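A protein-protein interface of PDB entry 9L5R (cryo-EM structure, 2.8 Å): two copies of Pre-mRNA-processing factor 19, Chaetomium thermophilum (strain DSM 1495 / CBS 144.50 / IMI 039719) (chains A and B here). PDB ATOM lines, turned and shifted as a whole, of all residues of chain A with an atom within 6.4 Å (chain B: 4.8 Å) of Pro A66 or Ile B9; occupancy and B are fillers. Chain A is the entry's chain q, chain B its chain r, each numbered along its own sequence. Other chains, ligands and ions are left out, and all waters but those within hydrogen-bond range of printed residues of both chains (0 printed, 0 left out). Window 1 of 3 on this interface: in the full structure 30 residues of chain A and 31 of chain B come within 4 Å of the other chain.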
ATOM      1  N   MET A   1       2.720   8.959   2.323  1.00  0.00           N
ATOM      2  CA  MET A   1       3.570  10.121   2.543  1.00  0.00           C
ATOM      3  C   MET A   1       4.969   9.888   1.980  1.00  0.00           C
ATOM      4  O   MET A   1       5.437   8.749   1.891  1.00  0.00           O
ATOM      5  CB  MET A   1       3.640  10.455   4.034  1.00  0.00           C
ATOM      6  CG  MET A   1       4.468   9.483   4.861  1.00  0.00           C
ATOM      7  SD  MET A   1       3.707   7.857   4.992  1.00  0.00           S
ATOM      8  CE  MET A   1       2.286   8.220   6.010  1.00  0.00           C
ATOM      9  N   ARG A  64      -6.133   2.130  11.892  1.00  0.00           N
ATOM     10  CA  ARG A  64      -6.567   1.382  10.722  1.00  0.00           C
ATOM     11  C   ARG A  64      -5.554   1.559   9.598  1.00  0.00           C
ATOM     12  O   ARG A  64      -5.173   2.694   9.290  1.00  0.00           O
ATOM     13  CB  ARG A  64      -7.946   1.837  10.261  1.00  0.00           C
ATOM     14  CG  ARG A  64      -9.098   1.105  10.927  1.00  0.00           C
ATOM     15  CD  ARG A  64      -9.447   1.739  12.256  1.00  0.00           C
ATOM     16  NE  ARG A  64      -9.836   3.135  12.103  1.00  0.00           N
ATOM     17  CZ  ARG A  64      -9.868   4.012  13.095  1.00  0.00           C
ATOM     18  NH1 ARG A  64      -9.547   3.670  14.331  1.00  0.00           N
ATOM     19  NH2 ARG A  64     -10.229   5.267  12.841  1.00  0.00           N
ATOM     20  N   PRO A  65      -5.076   0.470   8.995  1.00  0.00           N
ATOM     21  CA  PRO A  65      -4.121   0.601   7.899  1.00  0.00           C
ATOM     22  C   PRO A  65      -4.771   1.241   6.687  1.00  0.00           C
ATOM     23  O   PRO A  65      -5.983   1.081   6.457  1.00  0.00           O
ATOM     24  CB  PRO A  65      -3.710  -0.855   7.614  1.00  0.00           C
ATOM     25  CG  PRO A  65      -4.835  -1.668   8.144  1.00  0.00           C
ATOM     26  CD  PRO A  65      -5.352  -0.935   9.332  1.00  0.00           C
ATOM     27  N   PRO A  66      -4.006   1.980   5.879  1.00  0.00           N
ATOM     28  CA  PRO A  66      -4.599   2.676   4.731  1.00  0.00           C
ATOM     29  C   PRO A  66      -4.994   1.739   3.600  1.00  0.00           C
ATOM     30  O   PRO A  66      -4.269   1.604   2.609  1.00  0.00           O
ATOM     31  CB  PRO A  66      -3.488   3.639   4.294  1.00  0.00           C
ATOM     32  CG  PRO A  66      -2.232   3.017   4.784  1.00  0.00           C
ATOM     33  CD  PRO A  66      -2.584   2.320   6.062  1.00  0.00           C
ATOM     34  N   ASN A  67      -6.144   1.088   3.741  1.00  0.00           N
ATOM     35  CA  ASN A  67      -6.679   0.210   2.714  1.00  0.00           C
ATOM     36  C   ASN A  67      -7.886   0.857   2.048  1.00  0.00           C
ATOM     37  O   ASN A  67      -8.578   1.686   2.646  1.00  0.00           O
ATOM     38  CB  ASN A  67      -7.070  -1.149   3.302  1.00  0.00           C
ATOM     39  CG  ASN A  67      -5.907  -1.841   3.980  1.00  0.00           C
ATOM     40  OD1 ASN A  67      -6.010  -2.271   5.127  1.00  0.00           O
ATOM     41  ND2 ASN A  67      -4.783  -1.933   3.279  1.00  0.00           N
ATOM     42  N   PHE A  68      -8.126   0.467   0.794  1.00  0.00           N
ATOM     43  CA  PHE A  68      -9.223   1.034   0.015  1.00  0.00           C
ATOM     44  C   PHE A  68     -10.592   0.621   0.535  1.00  0.00           C
ATOM     45  O   PHE A  68     -11.577   1.312   0.258  1.00  0.00           O
ATOM     46  CB  PHE A  68      -9.086   0.621  -1.449  1.00  0.00           C
ATOM     47  CG  PHE A  68      -9.837   1.501  -2.403  1.00  0.00           C
ATOM     48  CD1 PHE A  68      -9.311   2.718  -2.804  1.00  0.00           C
ATOM     49  CD2 PHE A  68     -11.063   1.105  -2.912  1.00  0.00           C
ATOM     50  CE1 PHE A  68      -9.998   3.529  -3.689  1.00  0.00           C
ATOM     51  CE2 PHE A  68     -11.757   1.912  -3.795  1.00  0.00           C
ATOM     52  CZ  PHE A  68     -11.222   3.124  -4.185  1.00  0.00           C
ATOM     53  N   SER A  70     -11.654   0.793   3.507  1.00  0.00           N
ATOM     54  CA  SER A  70     -12.057   1.597   4.651  1.00  0.00           C
ATOM     55  C   SER A  70     -13.064   2.668   4.244  1.00  0.00           C
ATOM     56  O   SER A  70     -13.095   3.132   3.101  1.00  0.00           O
ATOM     57  CB  SER A  70     -10.840   2.255   5.299  1.00  0.00           C
ATOM     58  OG  SER A  70     -10.331   3.291   4.476  1.00  0.00           O
ATOM     59  N   PRO A  72     -13.348   6.001   5.097  1.00  0.00           N
ATOM     60  CA  PRO A  72     -12.811   7.234   4.477  1.00  0.00           C
ATOM     61  C   PRO A  72     -12.370   7.051   3.034  1.00  0.00           C
ATOM     62  O   PRO A  72     -12.667   7.903   2.185  1.00  0.00           O
ATOM     63  CB  PRO A  72     -11.630   7.617   5.379  1.00  0.00           C
ATOM     64  CG  PRO A  72     -11.799   6.878   6.614  1.00  0.00           C
ATOM     65  CD  PRO A  72     -12.689   5.714   6.388  1.00  0.00           C
ATOM     66  N   LEU B   2       0.776   8.923  11.182  1.00  0.00           N
ATOM     67  CA  LEU B   2      -0.673   8.856  11.108  1.00  0.00           C
ATOM     68  C   LEU B   2      -1.306   9.969  11.929  1.00  0.00           C
ATOM     69  O   LEU B   2      -0.697  10.503  12.861  1.00  0.00           O
ATOM     70  CB  LEU B   2      -1.191   7.501  11.603  1.00  0.00           C
ATOM     71  CG  LEU B   2      -0.783   6.282  10.774  1.00  0.00           C
ATOM     72  CD1 LEU B   2      -1.183   4.999  11.478  1.00  0.00           C
ATOM     73  CD2 LEU B   2      -1.397   6.351   9.386  1.00  0.00           C
ATOM     74  N   GLY B   7      -6.281   7.645  13.265  1.00  0.00           N
ATOM     75  CA  GLY B   7      -5.624   6.364  13.150  1.00  0.00           C
ATOM     76  C   GLY B   7      -5.332   5.934  11.730  1.00  0.00           C
ATOM     77  O   GLY B   7      -4.620   4.943  11.531  1.00  0.00           O
ATOM     78  N   GLU B   8      -5.847   6.650  10.741  1.00  0.00           N
ATOM     79  CA  GLU B   8      -5.590   6.374   9.338  1.00  0.00           C
ATOM     80  C   GLU B   8      -4.720   7.483   8.758  1.00  0.00           C
ATOM     81  O   GLU B   8      -4.290   8.402   9.463  1.00  0.00           O
ATOM     82  CB  GLU B   8      -6.904   6.243   8.566  1.00  0.00           C
ATOM     83  CG  GLU B   8      -7.956   5.404   9.272  1.00  0.00           C
ATOM     84  CD  GLU B   8      -8.906   4.725   8.303  1.00  0.00           C
ATOM     85  OE1 GLU B   8      -8.686   4.834   7.079  1.00  0.00           O
ATOM     86  OE2 GLU B   8      -9.873   4.086   8.766  1.00  0.00           O
ATOM     87  N   ILE B   9      -4.460   7.389   7.462  1.00  0.00           N
ATOM     88  CA  ILE B   9      -3.657   8.424   6.798  1.00  0.00           C
ATOM     89  C   ILE B   9      -4.494   9.688   6.642  1.00  0.00           C
ATOM     90  O   ILE B   9      -5.645   9.616   6.172  1.00  0.00           O
ATOM     91  CB  ILE B   9      -3.144   7.919   5.446  1.00  0.00           C
ATOM     92  CG1 ILE B   9      -4.254   7.213   4.666  1.00  0.00           C
ATOM     93  CG2 ILE B   9      -1.969   6.978   5.646  1.00  0.00           C
ATOM     94  CD1 ILE B   9      -4.008   7.136   3.181  1.00  0.00           C
ATOM     95  N   PRO B  10      -3.993  10.852   7.053  1.00  0.00           N
ATOM     96  CA  PRO B  10      -4.738  12.095   6.838  1.00  0.00           C
ATOM     97  C   PRO B  10      -4.471  12.687   5.464  1.00  0.00           C
ATOM     98  O   PRO B  10      -3.342  12.702   4.968  1.00  0.00           O
ATOM     99  CB  PRO B  10      -4.205  13.008   7.951  1.00  0.00           C
ATOM    100  CG  PRO B  10      -2.820  12.525   8.191  1.00  0.00           C
ATOM    101  CD  PRO B  10      -2.783  11.056   7.868  1.00  0.00           C
ATOM    102  N   GLU B  11      -5.539  13.173   4.833  1.00  0.00           N
ATOM    103  CA  GLU B  11      -5.428  13.744   3.498  1.00  0.00           C
ATOM    104  C   GLU B  11      -5.113  15.232   3.508  1.00  0.00           C
ATOM    105  O   GLU B  11      -4.551  15.738   2.530  1.00  0.00           O
ATOM    106  CB  GLU B  11      -6.714  13.500   2.704  1.00  0.00           C
ATOM    107  CG  GLU B  11      -6.896  12.055   2.270  1.00  0.00           C
ATOM    108  CD  GLU B  11      -7.869  11.909   1.119  1.00  0.00           C
ATOM    109  OE1 GLU B  11      -8.421  12.937   0.673  1.00  0.00           O
ATOM    110  OE2 GLU B  11      -8.080  10.767   0.658  1.00  0.00           O
ATOM    111  N   VAL B  60      -1.641  10.407  -0.708  1.00  0.00           N
ATOM    112  CA  VAL B  60      -1.284   9.026  -0.407  1.00  0.00           C
ATOM    113  C   VAL B  60      -2.257   8.104  -1.127  1.00  0.00           C
ATOM    114  O   VAL B  60      -3.478   8.225  -0.970  1.00  0.00           O
ATOM    115  CB  VAL B  60      -1.295   8.778   1.108  1.00  0.00           C
ATOM    116  CG1 VAL B  60      -0.699   7.415   1.422  1.00  0.00           C
ATOM    117  CG2 VAL B  60      -0.540   9.881   1.829  1.00  0.00           C
ATOM    118  N   ARG B  62      -4.227   4.797  -2.079  1.00  0.00           N
ATOM    119  CA  ARG B  62      -4.761   3.551  -1.552  1.00  0.00           C
ATOM    120  C   ARG B  62      -5.217   2.686  -2.715  1.00  0.00           C
ATOM    121  O   ARG B  62      -6.105   3.103  -3.474  1.00  0.00           O
ATOM    122  CB  ARG B  62      -5.920   3.825  -0.598  1.00  0.00           C
ATOM    123  CG  ARG B  62      -5.598   4.854   0.474  1.00  0.00           C
ATOM    124  CD  ARG B  62      -6.854   5.277   1.210  1.00  0.00           C
ATOM    125  NE  ARG B  62      -7.304   4.276   2.169  1.00  0.00           N
ATOM    126  CZ  ARG B  62      -7.420   4.488   3.473  1.00  0.00           C
ATOM    127  NH1 ARG B  62      -7.125   5.659   4.012  1.00  0.00           N
ATOM    128  NH2 ARG B  62      -7.863   3.507   4.253  1.00  0.00           N
ATOM    129  N   PRO B  63      -4.648   1.495  -2.903  1.00  0.00           N
ATOM    130  CA  PRO B  63      -4.907   0.733  -4.133  1.00  0.00           C
ATOM    131  C   PRO B  63      -6.275   0.066  -4.119  1.00  0.00           C
ATOM    132  O   PRO B  63      -6.642  -0.618  -3.161  1.00  0.00           O
ATOM    133  CB  PRO B  63      -3.783  -0.307  -4.148  1.00  0.00           C
ATOM    134  CG  PRO B  63      -3.426  -0.495  -2.712  1.00  0.00           C
ATOM    135  CD  PRO B  63      -3.703   0.807  -2.006  1.00  0.00           C
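The backbone carbonyl oxygen (O) of Asn A67 lies within hydrogen-bond range of the guanidinium group (NH2) of Arg B62. The backbone carbonyl oxygen of Gly B7 lies within hydrogen-bond range of the backbone NH of Arg A64, 3.2 Å away. The side-chain carboxylate (OE1) of Glu B8 sits at hydrogen-bond distance from the side-chain hydroxyl (OG) of Ser A70 (3.4 Å). OG of Ser A70 is in hydrogen-bond range of NH2 of Arg B62. The side-chain carboxylate (OE2) of Glu B8 is in salt-bridge range of the guanidinium group (NE) of Arg A64, 3.5 Å away.
The side-chain hydroxyl (OG) of Ser A70 lies within hydrogen-bond range of the backbone carbonyl oxygen (O) of Asn A67 (3.0 Å). The guanidinium group (NH2) of Arg B62 is in salt-bridge range of the side-chain carboxylate (OE1) of Glu B8, at 3.2 Å.
Among the printed residues, merely in contact across the chains: Phe A68 with Pro B63, Phe A68 with Arg B62, Pro A66 with Arg B62, Met A1 with Val B60, Pro A66 with Ile B9, Pro A72 with Glu B8 and Pro A65 with Arg B62.
Of chain B, only Ile B9 and Arg B62 come within 4 Å of Pro A66. Of chain A, only Pro A66 (3.7 Å) comes within 4 Å of Ile B9. Printed residues of chain B within 4 Å of Asn A67: Arg B62. Printed residues of chain B within 4 Å of Met A1: Val B60. Of the printed residues of chain A, Glu B8 touches Arg A64 (3.3 Å), Ser A70 (3.4 Å) and Pro A72 (3.8 Å). Of the printed residues of chain B, Ser A70 touches Glu B8 (3.4 Å) and Arg B62 (2.5 Å). The nearest residue of chain A that does not touch Ile B9 is Met A1 (4.4 Å). The nearest printed residue of chain B that does not touch Arg A64 is Ile B9 (5.1 Å).
Printed residues of chain B that touch a printed residue of chain A: Gly B7, Glu B8, Ile B9, Val B60, Arg B62 and Pro B63. Hydrophobic or aromatic side chains of chain B within 4 Å of the printed part of chain A: Ile B9 and Val B60. Of the 8 printed residues of chain A, 8 touch a printed residue of chain B. Printed residues of chain A that touch a printed residue of chain B: Met A1, Arg A64, Pro A65, Pro A66, Asn A67, Phe A68, Ser A70 and Pro A72. Hydrophobic or aromatic side chains of chain A that line the printed part of chain B: Pro A66, Phe A68 and Pro A72. Among the printed residues, 12 pairs touch across the chains.
No position is printed for both chains. Of the 12 pairs that touch across the chains among the printed residues, none has its exchanged pair printed and touching as well.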
